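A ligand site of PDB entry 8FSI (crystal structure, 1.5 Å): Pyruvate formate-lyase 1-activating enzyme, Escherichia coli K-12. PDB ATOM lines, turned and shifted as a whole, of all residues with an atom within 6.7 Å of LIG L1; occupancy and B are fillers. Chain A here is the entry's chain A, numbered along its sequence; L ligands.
A sulfur (S2) of LIG L1 sits close to the backbone NH of Cys 33. SG of Cys 33 binds FE1 of LIG L1, at 2.3 Å. An iron atom (FE3) of LIG L1 is bound by the side-chain sulfur of Cys 36, at 2.3 Å. An iron atom (FE4) of LIG L1 is bound by the side-chain sulfur (SG) of Cys 29. A sulfur (S2) of LIG L1 sits close to the indole nitrogen (NE1) of Trp 42 (3.3 Å). A sulfur (S3) of LIG L1 sits close to the side-chain amide nitrogen of Asn 106, 3.4 Å away. S1 of LIG L1 lies close to N of Gly 78 (3.5 Å). The side-chain amino group (NZ) of Lys 131 lies close to a sulfur (S4) of LIG L1 (3.7 Å). The backbone carbonyl oxygen (O) of Gly 78 lies close to a nitrogen (N1) of LG2 L2 (3.0 Å). The side-chain amino group of Lys 131 is in hydrogen-bond range of an oxygen (O5) of LG2 L2 (3.2 Å). The backbone carbonyl oxygen of Tyr 35 sits at hydrogen-bond distance from a nitrogen (N4) of LG2 L2 (2.8 Å). N1 of LG2 L2 lies close to OE1 of Glu 79 (3.3 Å). N of His 37 is in hydrogen-bond range of N3 of LG2 L2 (3.1 Å). NE2 of His 37 lies close to O3 of LG2 L2 (3.5 Å). OD2 of Asp 129 lies within hydrogen-bond range of O5 of LG2 L2.
An oxygen (O1) of LG2 L2 binds an iron atom (FE2) of LIG L1.
NE1 of Trp 42 lies close to SG of Cys 36, 3.5 Å away. The backbone NH of Cys 29 sits at hydrogen-bond distance from the backbone carbonyl oxygen of Trp 42 (3.0 Å). The side-chain sulfur (SG) of Cys 29 sits close to the backbone NH (N) of Met 31, at 3.5 Å. The guanidinium group of Arg 32 sits at hydrogen-bond distance from the backbone carbonyl oxygen of Cys 29 (2.9 Å). ND2 of Asn 106 sits at hydrogen-bond distance from SD of Met 31 (3.6 Å). OG1 of Thr 41 sits at hydrogen-bond distance from N of Gly 78. The side-chain hydroxyl (OH) of Tyr 35 lies close to the side-chain amino group (NZ) of Lys 131 (3.5 Å). The side-chain amino group (NZ) of Lys 131 lies within salt-bridge range of the side-chain carboxylate (OD2) of Asp 129, 3.0 Å away.
O of Met 31 lies close to S2 of LIG L1 (3.7 Å). Hydrophobic or aromatic side chains within 4 Å of LIG L1: Met 31 and Trp 42. Of the 22 residues printed, 8 come within 4 Å of LIG L1. Along chain A the residues within 4 Å of LIG L1 span positions 29 to 131. The nearest printed residue that does not touch LIG L1 is Thr 41 (4.1 Å).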
ATOM      1  N   GLY A  28     -22.355 -26.548 -17.459  1.00  0.00           N
ATOM      2  CA  GLY A  28     -22.473 -26.902 -18.856  1.00  0.00           C
ATOM      3  C   GLY A  28     -21.386 -26.228 -19.677  1.00  0.00           C
ATOM      4  O   GLY A  28     -21.153 -25.026 -19.556  1.00  0.00           O
ATOM      5  N   CYS A  29     -20.678 -27.047 -20.486  1.00  0.00           N
ATOM      6  CA  CYS A  29     -19.681 -26.562 -21.427  1.00  0.00           C
ATOM      7  C   CYS A  29     -19.665 -27.512 -22.601  1.00  0.00           C
ATOM      8  O   CYS A  29     -19.797 -28.731 -22.405  1.00  0.00           O
ATOM      9  CB  CYS A  29     -18.305 -26.521 -20.784  1.00  0.00           C
ATOM     10  SG  CYS A  29     -17.110 -25.690 -21.891  1.00  0.00           S
ATOM     11  N   LEU A  30     -19.496 -26.971 -23.811  1.00  0.00           N
ATOM     12  CA  LEU A  30     -19.435 -27.756 -25.027  1.00  0.00           C
ATOM     13  C   LEU A  30     -18.044 -27.840 -25.616  1.00  0.00           C
ATOM     14  O   LEU A  30     -17.895 -28.401 -26.699  1.00  0.00           O
ATOM     15  CB  LEU A  30     -20.428 -27.256 -26.061  1.00  0.00           C
ATOM     16  CG  LEU A  30     -21.871 -27.234 -25.577  1.00  0.00           C
ATOM     17  CD1 LEU A  30     -22.819 -26.774 -26.716  1.00  0.00           C
ATOM     18  CD2 LEU A  30     -22.326 -28.588 -25.058  1.00  0.00           C
ATOM     19  N   MET A  31     -17.014 -27.336 -24.925  1.00  0.00           N
ATOM     20  CA  MET A  31     -15.624 -27.619 -25.260  1.00  0.00           C
ATOM     21  C   MET A  31     -15.104 -28.754 -24.386  1.00  0.00           C
ATOM     22  O   MET A  31     -15.776 -29.243 -23.475  1.00  0.00           O
ATOM     23  CB  MET A  31     -14.767 -26.350 -25.147  1.00  0.00           C
ATOM     24  CG  MET A  31     -14.998 -25.371 -26.236  1.00  0.00           C
ATOM     25  SD  MET A  31     -13.842 -24.002 -26.136  1.00  0.00           S
ATOM     26  CE  MET A  31     -14.006 -23.269 -27.737  1.00  0.00           C
ATOM     27  N   ARG A  32     -13.914 -29.250 -24.721  1.00  0.00           N
ATOM     28  CA  ARG A  32     -13.378 -30.482 -24.163  1.00  0.00           C
ATOM     29  C   ARG A  32     -11.885 -30.347 -23.851  1.00  0.00           C
ATOM     30  O   ARG A  32     -11.116 -31.309 -24.000  1.00  0.00           O
ATOM     31  CB  ARG A  32     -13.652 -31.681 -25.095  1.00  0.00           C
ATOM     32  CG  ARG A  32     -15.134 -32.011 -25.302  1.00  0.00           C
ATOM     33  CD  ARG A  32     -15.787 -32.483 -24.029  1.00  0.00           C
ATOM     34  NE  ARG A  32     -17.202 -32.819 -24.191  1.00  0.00           N
ATOM     35  CZ  ARG A  32     -18.215 -32.086 -23.789  1.00  0.00           C
ATOM     36  NH1 ARG A  32     -18.035 -30.920 -23.224  1.00  0.00           N
ATOM     37  NH2 ARG A  32     -19.460 -32.547 -23.943  1.00  0.00           N
ATOM     38  N   CYS A  33     -11.487 -29.180 -23.385  1.00  0.00           N
ATOM     39  CA  CYS A  33     -10.067 -28.896 -23.181  1.00  0.00           C
ATOM     40  C   CYS A  33      -9.390 -29.969 -22.362  1.00  0.00           C
ATOM     41  O   CYS A  33      -9.831 -30.298 -21.251  1.00  0.00           O
ATOM     42  CB  CYS A  33      -9.951 -27.568 -22.406  1.00  0.00           C
ATOM     43  SG  CYS A  33     -10.794 -26.166 -23.135  1.00  0.00           S
ATOM     44  N   LEU A  34      -8.272 -30.481 -22.882  1.00  0.00           N
ATOM     45  CA  LEU A  34      -7.582 -31.574 -22.216  1.00  0.00           C
ATOM     46  C   LEU A  34      -7.123 -31.179 -20.813  1.00  0.00           C
ATOM     47  O   LEU A  34      -6.919 -32.043 -19.979  1.00  0.00           O
ATOM     48  CB  LEU A  34      -6.360 -32.007 -23.027  1.00  0.00           C
ATOM     49  CG  LEU A  34      -6.592 -32.457 -24.437  1.00  0.00           C
ATOM     50  CD1 LEU A  34      -5.274 -32.921 -25.048  1.00  0.00           C
ATOM     51  CD2 LEU A  34      -7.598 -33.620 -24.489  1.00  0.00           C
ATOM     52  N   TYR A  35      -6.943 -29.881 -20.578  1.00  0.00           N
ATOM     53  CA  TYR A  35      -6.457 -29.385 -19.309  1.00  0.00           C
ATOM     54  C   TYR A  35      -7.547 -28.961 -18.343  1.00  0.00           C
ATOM     55  O   TYR A  35      -7.208 -28.593 -17.229  1.00  0.00           O
ATOM     56  CB  TYR A  35      -5.508 -28.200 -19.556  1.00  0.00           C
ATOM     57  CG  TYR A  35      -5.988 -27.048 -20.426  1.00  0.00           C
ATOM     58  CD1 TYR A  35      -6.930 -26.153 -19.994  1.00  0.00           C
ATOM     59  CD2 TYR A  35      -5.446 -26.850 -21.684  1.00  0.00           C
ATOM     60  CE1 TYR A  35      -7.319 -25.080 -20.795  1.00  0.00           C
ATOM     61  CE2 TYR A  35      -5.806 -25.793 -22.486  1.00  0.00           C
ATOM     62  CZ  TYR A  35      -6.720 -24.918 -22.028  1.00  0.00           C
ATOM     63  OH  TYR A  35      -7.095 -23.816 -22.773  1.00  0.00           O
ATOM     64  N   CYS A  36      -8.807 -29.001 -18.723  1.00  0.00           N
ATOM     65  CA  CYS A  36      -9.841 -28.336 -17.938  1.00  0.00           C
ATOM     66  C   CYS A  36      -9.708 -28.647 -16.464  1.00  0.00           C
ATOM     67  O   CYS A  36      -9.798 -29.803 -16.040  1.00  0.00           O
ATOM     68  CB  CYS A  36     -11.206 -28.796 -18.391  1.00  0.00           C
ATOM     69  SG  CYS A  36     -12.530 -27.838 -17.570  1.00  0.00           S
ATOM     70  N   HIS A  37      -9.583 -27.620 -15.645  1.00  0.00           N
ATOM     71  CA  HIS A  37      -9.497 -27.810 -14.209  1.00  0.00           C
ATOM     72  C   HIS A  37     -10.854 -27.878 -13.522  1.00  0.00           C
ATOM     73  O   HIS A  37     -10.875 -28.070 -12.292  1.00  0.00           O
ATOM     74  CB  HIS A  37      -8.590 -26.779 -13.545  1.00  0.00           C
ATOM     75  CG  HIS A  37      -9.021 -25.366 -13.646  1.00  0.00           C
ATOM     76  ND1 HIS A  37      -8.131 -24.322 -13.546  1.00  0.00           N
ATOM     77  CD2 HIS A  37     -10.245 -24.810 -13.768  1.00  0.00           C
ATOM     78  CE1 HIS A  37      -8.784 -23.180 -13.621  1.00  0.00           C
ATOM     79  NE2 HIS A  37     -10.074 -23.438 -13.758  1.00  0.00           N
ATOM     80  N   ASN A  38     -11.944 -27.800 -14.292  1.00  0.00           N
ATOM     81  CA  ASN A  38     -13.315 -27.900 -13.811  1.00  0.00           C
ATOM     82  C   ASN A  38     -14.095 -28.972 -14.585  1.00  0.00           C
ATOM     83  O   ASN A  38     -15.163 -28.706 -15.136  1.00  0.00           O
ATOM     84  CB  ASN A  38     -14.069 -26.565 -13.916  1.00  0.00           C
ATOM     85  CG  ASN A  38     -13.556 -25.516 -12.963  1.00  0.00           C
ATOM     86  OD1 ASN A  38     -12.899 -25.820 -11.990  1.00  0.00           O
ATOM     87  ND2 ASN A  38     -13.938 -24.262 -13.203  1.00  0.00           N
ATOM     88  N   ARG A  39     -13.573 -30.206 -14.652  1.00  0.00           N
ATOM     89  CA  ARG A  39     -14.160 -31.224 -15.502  1.00  0.00           C
ATOM     90  C   ARG A  39     -15.604 -31.566 -15.122  1.00  0.00           C
ATOM     91  O   ARG A  39     -16.386 -31.975 -15.980  1.00  0.00           O
ATOM     92  CB  ARG A  39     -13.267 -32.483 -15.458  1.00  0.00           C
ATOM     93  CG  ARG A  39     -13.855 -33.737 -16.053  1.00  0.00           C
ATOM     94  CD  ARG A  39     -13.994 -33.600 -17.571  1.00  0.00           C
ATOM     95  NE  ARG A  39     -14.612 -34.777 -18.162  1.00  0.00           N
ATOM     96  CZ  ARG A  39     -15.916 -35.033 -18.113  1.00  0.00           C
ATOM     97  NH1 ARG A  39     -16.761 -34.271 -17.456  1.00  0.00           N
ATOM     98  NH2 ARG A  39     -16.389 -36.091 -18.772  1.00  0.00           N
ATOM     99  N   THR A  41     -17.958 -29.507 -14.584  1.00  0.00           N
ATOM    100  CA  THR A  41     -18.875 -28.484 -15.055  1.00  0.00           C
ATOM    101  C   THR A  41     -19.364 -28.736 -16.479  1.00  0.00           C
ATOM    102  O   THR A  41     -20.113 -27.920 -16.999  1.00  0.00           O
ATOM    103  CB  THR A  41     -18.230 -27.096 -15.045  1.00  0.00           C
ATOM    104  OG1 THR A  41     -17.145 -27.024 -15.980  1.00  0.00           O
ATOM    105  CG2 THR A  41     -17.747 -26.691 -13.676  1.00  0.00           C
ATOM    106  N   TRP A  42     -18.987 -29.852 -17.113  1.00  0.00           N
ATOM    107  CA  TRP A  42     -19.311 -30.006 -18.521  1.00  0.00           C
ATOM    108  C   TRP A  42     -20.761 -30.380 -18.784  1.00  0.00           C
ATOM    109  O   TRP A  42     -21.359 -29.858 -19.741  1.00  0.00           O
ATOM    110  CB  TRP A  42     -18.456 -31.077 -19.158  1.00  0.00           C
ATOM    111  CG  TRP A  42     -17.012 -30.773 -19.258  1.00  0.00           C
ATOM    112  CD1 TRP A  42     -16.358 -29.681 -18.772  1.00  0.00           C
ATOM    113  CD2 TRP A  42     -16.039 -31.593 -19.891  1.00  0.00           C
ATOM    114  NE1 TRP A  42     -15.020 -29.780 -19.079  1.00  0.00           N
ATOM    115  CE2 TRP A  42     -14.824 -30.920 -19.796  1.00  0.00           C
ATOM    116  CE3 TRP A  42     -16.092 -32.798 -20.579  1.00  0.00           C
ATOM    117  CZ2 TRP A  42     -13.637 -31.457 -20.303  1.00  0.00           C
ATOM    118  CZ3 TRP A  42     -14.916 -33.341 -21.101  1.00  0.00           C
ATOM    119  CH2 TRP A  42     -13.732 -32.646 -20.968  1.00  0.00           C
ATOM    120  N   GLY A  77     -17.575 -20.732 -15.150  1.00  0.00           N
ATOM    121  CA  GLY A  77     -18.101 -22.076 -15.284  1.00  0.00           C
ATOM    122  C   GLY A  77     -17.025 -23.093 -15.559  1.00  0.00           C
ATOM    123  O   GLY A  77     -15.936 -22.968 -14.992  1.00  0.00           O
ATOM    124  N   GLY A  78     -17.296 -24.120 -16.355  1.00  0.00           N
ATOM    125  CA  GLY A  78     -18.386 -24.181 -17.312  1.00  0.00           C
ATOM    126  C   GLY A  78     -18.319 -23.033 -18.276  1.00  0.00           C
ATOM    127  O   GLY A  78     -17.438 -22.136 -18.165  1.00  0.00           O
ATOM    128  N   GLU A  79     -19.292 -22.963 -19.185  1.00  0.00           N
ATOM    129  CA  GLU A  79     -19.396 -21.904 -20.163  1.00  0.00           C
ATOM    130  C   GLU A  79     -20.672 -21.097 -20.003  1.00  0.00           C
ATOM    131  O   GLU A  79     -21.762 -21.548 -20.393  1.00  0.00           O
ATOM    132  CB  GLU A  79     -19.303 -22.384 -21.594  1.00  0.00           C
ATOM    133  CG  GLU A  79     -19.344 -21.265 -22.573  1.00  0.00           C
ATOM    134  CD  GLU A  79     -18.439 -20.084 -22.192  1.00  0.00           C
ATOM    135  OE1 GLU A  79     -17.246 -20.323 -21.890  1.00  0.00           O
ATOM    136  OE2 GLU A  79     -18.943 -18.927 -22.109  1.00  0.00           O
ATOM    137  N   THR A 105     -15.335 -16.341 -20.542  1.00  0.00           N
ATOM    138  CA  THR A 105     -15.910 -17.130 -21.627  1.00  0.00           C
ATOM    139  C   THR A 105     -14.899 -17.715 -22.579  1.00  0.00           C
ATOM    140  O   THR A 105     -13.829 -17.156 -22.824  1.00  0.00           O
ATOM    141  CB  THR A 105     -16.954 -16.298 -22.422  1.00  0.00           C
ATOM    142  OG1 THR A 105     -17.613 -17.031 -23.458  1.00  0.00           O
ATOM    143  CG2 THR A 105     -16.327 -15.082 -23.108  1.00  0.00           C
ATOM    144  N   ASN A 106     -15.288 -18.876 -23.130  1.00  0.00           N
ATOM    145  CA  ASN A 106     -14.576 -19.502 -24.229  1.00  0.00           C
ATOM    146  C   ASN A 106     -15.018 -18.960 -25.592  1.00  0.00           C
ATOM    147  O   ASN A 106     -14.465 -19.351 -26.610  1.00  0.00           O
ATOM    148  CB  ASN A 106     -14.770 -21.021 -24.207  1.00  0.00           C
ATOM    149  CG  ASN A 106     -16.220 -21.488 -24.435  1.00  0.00           C
ATOM    150  OD1 ASN A 106     -17.060 -20.754 -24.951  1.00  0.00           O
ATOM    151  ND2 ASN A 106     -16.490 -22.755 -24.087  1.00  0.00           N
ATOM    152  N   ASP A 129     -11.046 -16.439 -23.577  1.00  0.00           N
ATOM    153  CA  ASP A 129      -9.959 -17.379 -23.889  1.00  0.00           C
ATOM    154  C   ASP A 129      -9.781 -17.533 -25.399  1.00  0.00           C
ATOM    155  O   ASP A 129     -10.745 -17.755 -26.141  1.00  0.00           O
ATOM    156  CB  ASP A 129     -10.257 -18.778 -23.370  1.00  0.00           C
ATOM    157  CG  ASP A 129      -9.615 -19.065 -22.051  1.00  0.00           C
ATOM    158  OD1 ASP A 129      -9.686 -18.222 -21.141  1.00  0.00           O
ATOM    159  OD2 ASP A 129      -9.001 -20.146 -21.895  1.00  0.00           O
ATOM    160  N   LYS A 131      -7.611 -20.144 -27.074  1.00  0.00           N
ATOM    161  CA  LYS A 131      -6.878 -21.299 -26.553  1.00  0.00           C
ATOM    162  C   LYS A 131      -5.778 -21.770 -27.483  1.00  0.00           C
ATOM    163  O   LYS A 131      -4.822 -22.385 -27.015  1.00  0.00           O
ATOM    164  CB  LYS A 131      -7.825 -22.442 -26.234  1.00  0.00           C
ATOM    165  CG  LYS A 131      -8.862 -22.046 -25.142  1.00  0.00           C
ATOM    166  CD  LYS A 131      -9.870 -23.123 -24.907  1.00  0.00           C
ATOM    167  CE  LYS A 131     -10.927 -22.666 -23.914  1.00  0.00           C
ATOM    168  NZ  LYS A 131     -10.392 -22.681 -22.497  1.00  0.00           N
ATOM    169  N   VAL A 142      -8.818 -29.142 -27.675  1.00  0.00           N
ATOM    170  CA  VAL A 142     -10.107 -28.678 -27.185  1.00  0.00           C
ATOM    171  C   VAL A 142     -11.272 -29.480 -27.722  1.00  0.00           C
ATOM    172  O   VAL A 142     -12.373 -29.431 -27.127  1.00  0.00           O
ATOM    173  CB  VAL A 142     -10.273 -27.181 -27.562  1.00  0.00           C
ATOM    174  CG1 VAL A 142     -11.566 -26.599 -27.038  1.00  0.00           C
ATOM    175  CG2 VAL A 142      -9.113 -26.338 -27.076  1.00  0.00           C
HETATM  176 FE1  LIG L   1     -12.400 -25.663 -21.618  1.00  0.00          FE
HETATM  177 FE2  LIG L   1     -13.531 -23.596 -20.105  1.00  0.00          FE
HETATM  178 FE3  LIG L   1     -13.133 -26.284 -19.118  1.00  0.00          FE
HETATM  179 FE4  LIG L   1     -15.029 -25.752 -20.942  1.00  0.00          FE
HETATM  180  S1  LIG L   1     -14.944 -25.024 -18.776  1.00  0.00           S
HETATM  181  S2  LIG L   1     -13.641 -27.476 -21.048  1.00  0.00           S
HETATM  182  S3  LIG L   1     -13.953 -24.189 -22.270  1.00  0.00           S
HETATM  183  S4  LIG L   1     -11.517 -24.731 -19.694  1.00  0.00           S
HETATM  184  N1  LG2 L   2     -15.081 -21.963 -19.956  1.00  0.00           N
HETATM  185  C1  LG2 L   2     -14.492 -20.634 -19.822  1.00  0.00           C
HETATM  186  C2  LG2 L   2     -13.124 -20.684 -20.421  1.00  0.00           C
HETATM  187  O1  LG2 L   2     -12.541 -21.750 -20.644  1.00  0.00           O
HETATM  188  O2  LG2 L   2     -12.579 -19.590 -20.650  1.00  0.00           O
HETATM  189  C3  LG2 L   2     -14.500 -20.209 -18.340  1.00  0.00           C
HETATM  190  C4  LG2 L   2     -14.202 -21.282 -17.299  1.00  0.00           C
HETATM  191  S1  LG2 L   2     -12.481 -21.826 -17.305  1.00  0.00           S
HETATM  192  C5  LG2 L   2     -12.494 -23.149 -16.046  1.00  0.00           C
HETATM  193  C6  LG2 L   2     -11.652 -20.436 -16.470  1.00  0.00           C
HETATM  194  C7  LG2 L   2     -10.219 -20.256 -16.921  1.00  0.00           C
HETATM  195  O3  LG2 L   2      -9.394 -21.349 -16.436  1.00  0.00           O
HETATM  196  C8  LG2 L   2      -9.963 -20.263 -18.439  1.00  0.00           C
HETATM  197  O4  LG2 L   2      -9.077 -19.175 -18.784  1.00  0.00           O
HETATM  198  C9  LG2 L   2      -9.377 -21.620 -18.732  1.00  0.00           C
HETATM  199  O5  LG2 L   2      -8.671 -21.762 -19.910  1.00  0.00           O
HETATM  200  C10 LG2 L   2      -8.499 -21.746 -17.469  1.00  0.00           C
HETATM  201  N2  LG2 L   2      -8.002 -23.072 -17.179  1.00  0.00           N
HETATM  202  C11 LG2 L   2      -8.748 -24.188 -17.249  1.00  0.00           C
HETATM  203  N3  LG2 L   2      -8.014 -25.277 -16.932  1.00  0.00           N
HETATM  204  C12 LG2 L   2      -6.722 -24.809 -16.660  1.00  0.00           C
HETATM  205  C13 LG2 L   2      -5.519 -25.415 -16.288  1.00  0.00           C
HETATM  206  N4  LG2 L   2      -5.417 -26.719 -16.118  1.00  0.00           N
HETATM  207  N5  LG2 L   2      -4.443 -24.593 -16.117  1.00  0.00           N
HETATM  208  C14 LG2 L   2      -4.502 -23.247 -16.257  1.00  0.00           C
HETATM  209  N6  LG2 L   2      -5.682 -22.601 -16.621  1.00  0.00           N
HETATM  210  C15 LG2 L   2      -6.722 -23.429 -16.828  1.00  0.00           C
